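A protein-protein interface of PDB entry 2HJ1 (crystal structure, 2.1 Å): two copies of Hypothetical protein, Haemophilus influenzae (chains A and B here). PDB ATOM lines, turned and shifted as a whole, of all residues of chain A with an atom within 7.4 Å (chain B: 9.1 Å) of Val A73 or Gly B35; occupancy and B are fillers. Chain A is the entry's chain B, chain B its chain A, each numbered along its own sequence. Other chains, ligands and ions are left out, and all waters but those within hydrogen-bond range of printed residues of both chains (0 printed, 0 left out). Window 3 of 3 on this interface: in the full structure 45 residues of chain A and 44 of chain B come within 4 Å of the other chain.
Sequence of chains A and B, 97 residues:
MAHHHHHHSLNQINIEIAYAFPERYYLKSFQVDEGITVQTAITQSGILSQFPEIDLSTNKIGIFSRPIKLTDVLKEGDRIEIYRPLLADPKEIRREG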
ATOM      1  N   LYS A  69      -9.131  15.927  11.194  1.00  0.00           N
ATOM      2  CA  LYS A  69      -9.458  15.779  12.603  1.00  0.00           C
ATOM      3  C   LYS A  69      -9.446  17.195  13.116  1.00  0.00           C
ATOM      4  O   LYS A  69      -8.588  18.006  12.712  1.00  0.00           O
ATOM      5  CB  LYS A  69      -8.396  14.927  13.272  1.00  0.00           C
ATOM      6  CG  LYS A  69      -8.169  13.608  12.499  1.00  0.00           C
ATOM      7  CD  LYS A  69      -7.514  12.551  13.348  1.00  0.00           C
ATOM      8  CE  LYS A  69      -6.024  12.793  13.487  1.00  0.00           C
ATOM      9  NZ  LYS A  69      -5.265  11.892  12.553  1.00  0.00           N
ATOM     10  N   LEU A  70     -10.412  17.536  13.945  1.00  0.00           N
ATOM     11  CA  LEU A  70     -10.434  18.882  14.538  1.00  0.00           C
ATOM     12  C   LEU A  70      -9.292  19.154  15.530  1.00  0.00           C
ATOM     13  O   LEU A  70      -9.108  20.270  16.000  1.00  0.00           O
ATOM     14  CB  LEU A  70     -11.779  19.153  15.195  1.00  0.00           C
ATOM     15  CG  LEU A  70     -12.969  19.062  14.239  1.00  0.00           C
ATOM     16  CD1 LEU A  70     -14.249  19.480  14.982  1.00  0.00           C
ATOM     17  CD2 LEU A  70     -12.761  19.835  12.942  1.00  0.00           C
ATOM     18  N   THR A  71      -8.520  18.115  15.824  1.00  0.00           N
ATOM     19  CA  THR A  71      -7.342  18.237  16.667  1.00  0.00           C
ATOM     20  C   THR A  71      -6.075  18.628  15.864  1.00  0.00           C
ATOM     21  O   THR A  71      -5.025  18.872  16.473  1.00  0.00           O
ATOM     22  CB  THR A  71      -7.066  16.886  17.390  1.00  0.00           C
ATOM     23  OG1 THR A  71      -7.053  15.833  16.418  1.00  0.00           O
ATOM     24  CG2 THR A  71      -8.158  16.604  18.408  1.00  0.00           C
ATOM     25  N   ASP A  72      -6.158  18.638  14.524  1.00  0.00           N
ATOM     26  CA  ASP A  72      -5.029  19.040  13.653  1.00  0.00           C
ATOM     27  C   ASP A  72      -4.542  20.458  13.987  1.00  0.00           C
ATOM     28  O   ASP A  72      -5.344  21.325  14.306  1.00  0.00           O
ATOM     29  CB  ASP A  72      -5.435  18.998  12.170  1.00  0.00           C
ATOM     30  CG  ASP A  72      -5.557  17.560  11.615  1.00  0.00           C
ATOM     31  OD1 ASP A  72      -5.262  16.557  12.341  1.00  0.00           O
ATOM     32  OD2 ASP A  72      -5.964  17.438  10.429  1.00  0.00           O
ATOM     33  N   VAL A  73      -3.230  20.684  13.917  1.00  0.00           N
ATOM     34  CA  VAL A  73      -2.636  21.995  14.278  1.00  0.00           C
ATOM     35  C   VAL A  73      -2.703  22.938  13.061  1.00  0.00           C
ATOM     36  O   VAL A  73      -2.398  22.526  11.946  1.00  0.00           O
ATOM     37  CB  VAL A  73      -1.184  21.834  14.877  1.00  0.00           C
ATOM     38  CG1 VAL A  73      -0.461  23.165  15.012  1.00  0.00           C
ATOM     39  CG2 VAL A  73      -1.262  21.187  16.260  1.00  0.00           C
ATOM     40  N   LEU A  74      -3.153  24.169  13.260  1.00  0.00           N
ATOM     41  CA  LEU A  74      -3.182  25.132  12.151  1.00  0.00           C
ATOM     42  C   LEU A  74      -1.809  25.733  11.869  1.00  0.00           C
ATOM     43  O   LEU A  74      -0.954  25.789  12.761  1.00  0.00           O
ATOM     44  CB  LEU A  74      -4.176  26.253  12.418  1.00  0.00           C
ATOM     45  CG  LEU A  74      -5.625  25.764  12.374  1.00  0.00           C
ATOM     46  CD1 LEU A  74      -6.434  26.732  13.181  1.00  0.00           C
ATOM     47  CD2 LEU A  74      -6.155  25.687  10.941  1.00  0.00           C
ATOM     48  N   LYS A  75      -1.629  26.186  10.628  1.00  0.00           N
ATOM     49  CA  LYS A  75      -0.408  26.841  10.182  1.00  0.00           C
ATOM     50  C   LYS A  75      -0.742  28.205   9.601  1.00  0.00           C
ATOM     51  O   LYS A  75      -1.908  28.502   9.260  1.00  0.00           O
ATOM     52  CB  LYS A  75       0.331  25.947   9.186  1.00  0.00           C
ATOM     53  CG  LYS A  75       1.094  24.794   9.882  1.00  0.00           C
ATOM     54  CD  LYS A  75       1.391  23.569   8.970  1.00  0.00           C
ATOM     55  CE  LYS A  75       2.712  23.698   8.124  1.00  0.00           C
ATOM     56  NZ  LYS A  75       3.136  22.395   7.450  1.00  0.00           N
ATOM     57  N   ASP A  78      -3.626  29.244   6.889  1.00  0.00           N
ATOM     58  CA  ASP A  78      -4.688  28.226   6.769  1.00  0.00           C
ATOM     59  C   ASP A  78      -6.058  28.885   6.762  1.00  0.00           C
ATOM     60  O   ASP A  78      -6.292  29.873   7.462  1.00  0.00           O
ATOM     61  CB  ASP A  78      -4.617  27.188   7.875  1.00  0.00           C
ATOM     62  CG  ASP A  78      -3.599  26.093   7.593  1.00  0.00           C
ATOM     63  OD1 ASP A  78      -3.045  25.985   6.458  1.00  0.00           O
ATOM     64  OD2 ASP A  78      -3.327  25.315   8.536  1.00  0.00           O
ATOM     65  N   ASN B  11       3.130  34.519  20.260  1.00  0.00           N
ATOM     66  CA  ASN B  11       3.704  34.110  18.934  1.00  0.00           C
ATOM     67  C   ASN B  11       2.587  33.631  17.986  1.00  0.00           C
ATOM     68  O   ASN B  11       2.049  32.535  18.172  1.00  0.00           O
ATOM     69  CB  ASN B  11       4.745  33.002  19.125  1.00  0.00           C
ATOM     70  CG  ASN B  11       5.643  32.820  17.899  1.00  0.00           C
ATOM     71  OD1 ASN B  11       6.836  32.499  18.026  1.00  0.00           O
ATOM     72  ND2 ASN B  11       5.079  33.043  16.707  1.00  0.00           N
ATOM     73  N   GLN B  12       2.260  34.449  16.982  1.00  0.00           N
ATOM     74  CA  GLN B  12       0.935  34.410  16.360  1.00  0.00           C
ATOM     75  C   GLN B  12       0.944  33.933  14.916  1.00  0.00           C
ATOM     76  O   GLN B  12       1.975  34.001  14.251  1.00  0.00           O
ATOM     77  CB  GLN B  12       0.300  35.802  16.406  1.00  0.00           C
ATOM     78  CG  GLN B  12       0.183  36.389  17.797  1.00  0.00           C
ATOM     79  CD  GLN B  12      -0.998  35.844  18.576  1.00  0.00           C
ATOM     80  OE1 GLN B  12      -2.114  36.354  18.459  1.00  0.00           O
ATOM     81  NE2 GLN B  12      -0.758  34.811  19.383  1.00  0.00           N
ATOM     82  N   ILE B  13      -0.202  33.442  14.436  1.00  0.00           N
ATOM     83  CA  ILE B  13      -0.365  33.136  12.999  1.00  0.00           C
ATOM     84  C   ILE B  13      -1.654  33.738  12.479  1.00  0.00           C
ATOM     85  O   ILE B  13      -2.574  33.963  13.241  1.00  0.00           O
ATOM     86  CB  ILE B  13      -0.300  31.617  12.675  1.00  0.00           C
ATOM     87  CG1 ILE B  13      -1.321  30.826  13.532  1.00  0.00           C
ATOM     88  CG2 ILE B  13       1.143  31.095  12.790  1.00  0.00           C
ATOM     89  CD1 ILE B  13      -1.669  29.435  13.010  1.00  0.00           C
ATOM     90  N   ILE B  15      -4.983  33.297  10.248  1.00  0.00           N
ATOM     91  CA  ILE B  15      -5.843  32.257   9.691  1.00  0.00           C
ATOM     92  C   ILE B  15      -7.148  32.846   9.298  1.00  0.00           C
ATOM     93  O   ILE B  15      -7.488  33.974   9.681  1.00  0.00           O
ATOM     94  CB  ILE B  15      -6.126  31.090  10.704  1.00  0.00           C
ATOM     95  CG1 ILE B  15      -6.846  31.616  11.962  1.00  0.00           C
ATOM     96  CG2 ILE B  15      -4.852  30.331  10.995  1.00  0.00           C
ATOM     97  CD1 ILE B  15      -7.508  30.552  12.824  1.00  0.00           C
ATOM     98  N   VAL B  32      -4.103  34.070  15.850  1.00  0.00           N
ATOM     99  CA  VAL B  32      -4.230  33.120  16.951  1.00  0.00           C
ATOM    100  C   VAL B  32      -2.847  32.617  17.309  1.00  0.00           C
ATOM    101  O   VAL B  32      -1.914  32.773  16.511  1.00  0.00           O
ATOM    102  CB  VAL B  32      -5.149  31.910  16.574  1.00  0.00           C
ATOM    103  CG1 VAL B  32      -6.590  32.383  16.394  1.00  0.00           C
ATOM    104  CG2 VAL B  32      -4.655  31.209  15.305  1.00  0.00           C
ATOM    105  N   ASP B  33      -2.731  31.994  18.479  1.00  0.00           N
ATOM    106  CA  ASP B  33      -1.478  31.401  18.916  1.00  0.00           C
ATOM    107  C   ASP B  33      -1.046  30.294  17.983  1.00  0.00           C
ATOM    108  O   ASP B  33      -1.792  29.342  17.735  1.00  0.00           O
ATOM    109  CB  ASP B  33      -1.600  30.800  20.325  1.00  0.00           C
ATOM    110  CG  ASP B  33      -1.955  31.834  21.384  1.00  0.00           C
ATOM    111  OD1 ASP B  33      -1.532  33.020  21.246  1.00  0.00           O
ATOM    112  OD2 ASP B  33      -2.669  31.451  22.352  1.00  0.00           O
ATOM    113  N   GLU B  34       0.174  30.409  17.483  1.00  0.00           N
ATOM    114  CA  GLU B  34       0.838  29.285  16.856  1.00  0.00           C
ATOM    115  C   GLU B  34       0.573  28.016  17.691  1.00  0.00           C
ATOM    116  O   GLU B  34       0.600  28.069  18.917  1.00  0.00           O
ATOM    117  CB  GLU B  34       2.323  29.596  16.792  1.00  0.00           C
ATOM    118  CG  GLU B  34       3.167  28.569  16.087  1.00  0.00           C
ATOM    119  CD  GLU B  34       4.536  29.146  15.693  1.00  0.00           C
ATOM    120  OE1 GLU B  34       4.720  29.477  14.488  1.00  0.00           O
ATOM    121  OE2 GLU B  34       5.404  29.285  16.599  1.00  0.00           O
ATOM    122  N   GLY B  35       0.298  26.892  17.030  1.00  0.00           N
ATOM    123  CA  GLY B  35       0.028  25.627  17.716  1.00  0.00           C
ATOM    124  C   GLY B  35      -1.433  25.296  18.009  1.00  0.00           C
ATOM    125  O   GLY B  35      -1.746  24.168  18.389  1.00  0.00           O
ATOM    126  N   ILE B  36      -2.319  26.275  17.847  1.00  0.00           N
ATOM    127  CA  ILE B  36      -3.772  26.096  18.014  1.00  0.00           C
ATOM    128  C   ILE B  36      -4.330  24.986  17.065  1.00  0.00           C
ATOM    129  O   ILE B  36      -3.872  24.844  15.919  1.00  0.00           O
ATOM    130  CB  ILE B  36      -4.499  27.481  17.816  1.00  0.00           C
ATOM    131  CG1 ILE B  36      -5.957  27.452  18.233  1.00  0.00           C
ATOM    132  CG2 ILE B  36      -4.424  27.977  16.375  1.00  0.00           C
ATOM    133  CD1 ILE B  36      -6.668  28.800  18.030  1.00  0.00           C
ATOM    134  N   THR B  37      -5.287  24.191  17.561  1.00  0.00           N
ATOM    135  CA  THR B  37      -5.967  23.184  16.749  1.00  0.00           C
ATOM    136  C   THR B  37      -7.112  23.809  16.000  1.00  0.00           C
ATOM    137  O   THR B  37      -7.519  24.919  16.303  1.00  0.00           O
ATOM    138  CB  THR B  37      -6.523  22.025  17.602  1.00  0.00           C
ATOM    139  OG1 THR B  37      -7.514  22.528  18.519  1.00  0.00           O
ATOM    140  CG2 THR B  37      -5.382  21.309  18.361  1.00  0.00           C
ATOM    141  N   VAL B  38      -7.616  23.105  14.987  1.00  0.00           N
ATOM    142  CA  VAL B  38      -8.788  23.575  14.246  1.00  0.00           C
ATOM    143  C   VAL B  38      -9.961  23.837  15.196  1.00  0.00           C
ATOM    144  O   VAL B  38     -10.651  24.855  15.088  1.00  0.00           O
ATOM    145  CB  VAL B  38      -9.234  22.526  13.186  1.00  0.00           C
ATOM    146  CG1 VAL B  38     -10.547  22.943  12.529  1.00  0.00           C
ATOM    147  CG2 VAL B  38      -8.084  22.291  12.172  1.00  0.00           C
ATOM    148  N   GLN B  39     -10.204  22.921  16.134  1.00  0.00           N
ATOM    149  CA  GLN B  39     -11.363  23.044  17.020  1.00  0.00           C
ATOM    150  C   GLN B  39     -11.264  24.277  17.888  1.00  0.00           C
ATOM    151  O   GLN B  39     -12.266  24.958  18.130  1.00  0.00           O
ATOM    152  CB  GLN B  39     -11.449  21.820  17.941  1.00  0.00           C
ATOM    153  CG  GLN B  39     -12.827  21.527  18.572  1.00  0.00           C
ATOM    154  CD  GLN B  39     -12.873  20.074  19.107  1.00  0.00           C
ATOM    155  OE1 GLN B  39     -13.603  19.246  18.607  1.00  0.00           O
ATOM    156  NE2 GLN B  39     -12.015  19.776  20.063  1.00  0.00           N
ATOM    157  N   THR B  40     -10.071  24.548  18.398  1.00  0.00           N
ATOM    158  CA  THR B  40      -9.884  25.691  19.307  1.00  0.00           C
ATOM    159  C   THR B  40     -10.142  26.974  18.521  1.00  0.00           C
ATOM    160  O   THR B  40     -10.849  27.864  18.998  1.00  0.00           O
ATOM    161  CB  THR B  40      -8.451  25.700  19.896  1.00  0.00           C
ATOM    162  OG1 THR B  40      -8.256  24.514  20.673  1.00  0.00           O
ATOM    163  CG2 THR B  40      -8.203  26.903  20.779  1.00  0.00           C
ATOM    164  N   ALA B  41      -9.623  27.024  17.278  1.00  0.00           N
ATOM    165  CA  ALA B  41      -9.853  28.165  16.403  1.00  0.00           C
ATOM    166  C   ALA B  41     -11.339  28.371  16.191  1.00  0.00           C
ATOM    167  O   ALA B  41     -11.829  29.493  16.251  1.00  0.00           O
ATOM    168  CB  ALA B  41      -9.101  27.985  15.033  1.00  0.00           C
ATOM    169  N   ILE B  63      -9.560  22.216   5.380  1.00  0.00           N
ATOM    170  CA  ILE B  63      -8.546  23.211   5.668  1.00  0.00           C
ATOM    171  C   ILE B  63      -7.841  23.464   4.347  1.00  0.00           C
ATOM    172  O   ILE B  63      -7.275  22.544   3.736  1.00  0.00           O
ATOM    173  CB  ILE B  63      -7.489  22.644   6.648  1.00  0.00           C
ATOM    174  CG1 ILE B  63      -8.087  22.153   7.987  1.00  0.00           C
ATOM    175  CG2 ILE B  63      -6.296  23.578   6.863  1.00  0.00           C
ATOM    176  CD1 ILE B  63      -8.814  23.186   8.781  1.00  0.00           C
ATOM    177  N   SER B  65      -4.595  25.064   2.718  1.00  0.00           N
ATOM    178  CA  SER B  65      -3.231  25.476   3.052  1.00  0.00           C
ATOM    179  C   SER B  65      -2.476  25.961   1.785  1.00  0.00           C
ATOM    180  O   SER B  65      -2.532  25.291   0.769  1.00  0.00           O
ATOM    181  CB  SER B  65      -2.428  24.300   3.610  1.00  0.00           C
ATOM    182  OG  SER B  65      -2.995  23.844   4.841  1.00  0.00           O
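O of Ile B36 lies within hydrogen-bond range of N of Leu A74, 2.8 Å away. N of Val B38 sits at hydrogen-bond distance from O of Leu A70, at 3.4 Å. N of Val B38 lies within hydrogen-bond range of O of Asp A72 (3.0 Å). N of Gln B39 lies within hydrogen-bond range of O of Leu A70 (2.9 Å). OD1 of Asp A78 is in hydrogen-bond range of OG of Ser B65 (2.7 Å).
The backbone carbonyl oxygen of Val B32 lies within hydrogen-bond range of the backbone NH of Ile B13 (2.8 Å). The side-chain hydroxyl (OG1) of Thr B40 lies within hydrogen-bond range of the side-chain hydroxyl (OG1) of Thr B37 (3.0 Å). The backbone NH of Lys A75 is in hydrogen-bond range of the side-chain carboxylate of Asp A78.
Thr B37 touches Leu A70 (CB to O, 3.5 Å). O of Thr A71 touches CG2 of Thr B37, 3.1 Å away. CA of Thr B37 touches O of Asp A72 (3.1 Å). CD1 of Ile B13 touches O of Leu A74, at 3.7 Å. Leu A74 touches Ile B15. CD1 of Leu A74 touches O of Thr B37, 3.8 Å away. Leu A74 touches Ala B41 (CD1 to CB, 3.5 Å). Lys A75 touches Ile B13 (C to CD1, 3.7 Å). CG2 of Ile B15 touches O of Lys A75, 3.9 Å away. Asp A78 touches Ile B63.
Printed residues of chain B within 4 Å of Leu A70: Thr B37 (3.5 Å), Val B38 (3.4 Å) and Gln B39 (2.9 Å). Of the printed residues of chain A, Ile B13 touches Leu A74 (3.7 Å) and Lys A75 (3.7 Å). Of the printed residues of chain A, Ile B15 touches Leu A74, Lys A75 and Asp A78. Asp B33 touches none of the printed residues of chain A. Glu B34 touches none of the printed residues of chain A. Gly B35 touches just one residue of chain A: Val A73 (3.7 Å). Printed residues of chain A within 4 Å of Ile B63: Asp A78. The nearest residue of chain B that does not touch Val A73 is Thr B37 (4.3 Å). The nearest printed residue of chain A that does not touch Ile B15 is Val A73 (8.0 Å).
Along chain B the printed residues that touch a printed residue of chain A span positions 13 to 65. Of the 8 printed residues of chain A, 7 touch a printed residue of chain B. Hydrophobic or aromatic side chains of chain A that line the printed part of chain B: Leu A70, Val A73 and Leu A74. Among the printed residues, 18 pairs touch across the chains. Among the printed residues, no Asp or Glu carboxylate lies within 4 Å of a Lys or Arg side-chain nitrogen of the other chain.
No position is printed for both chains.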
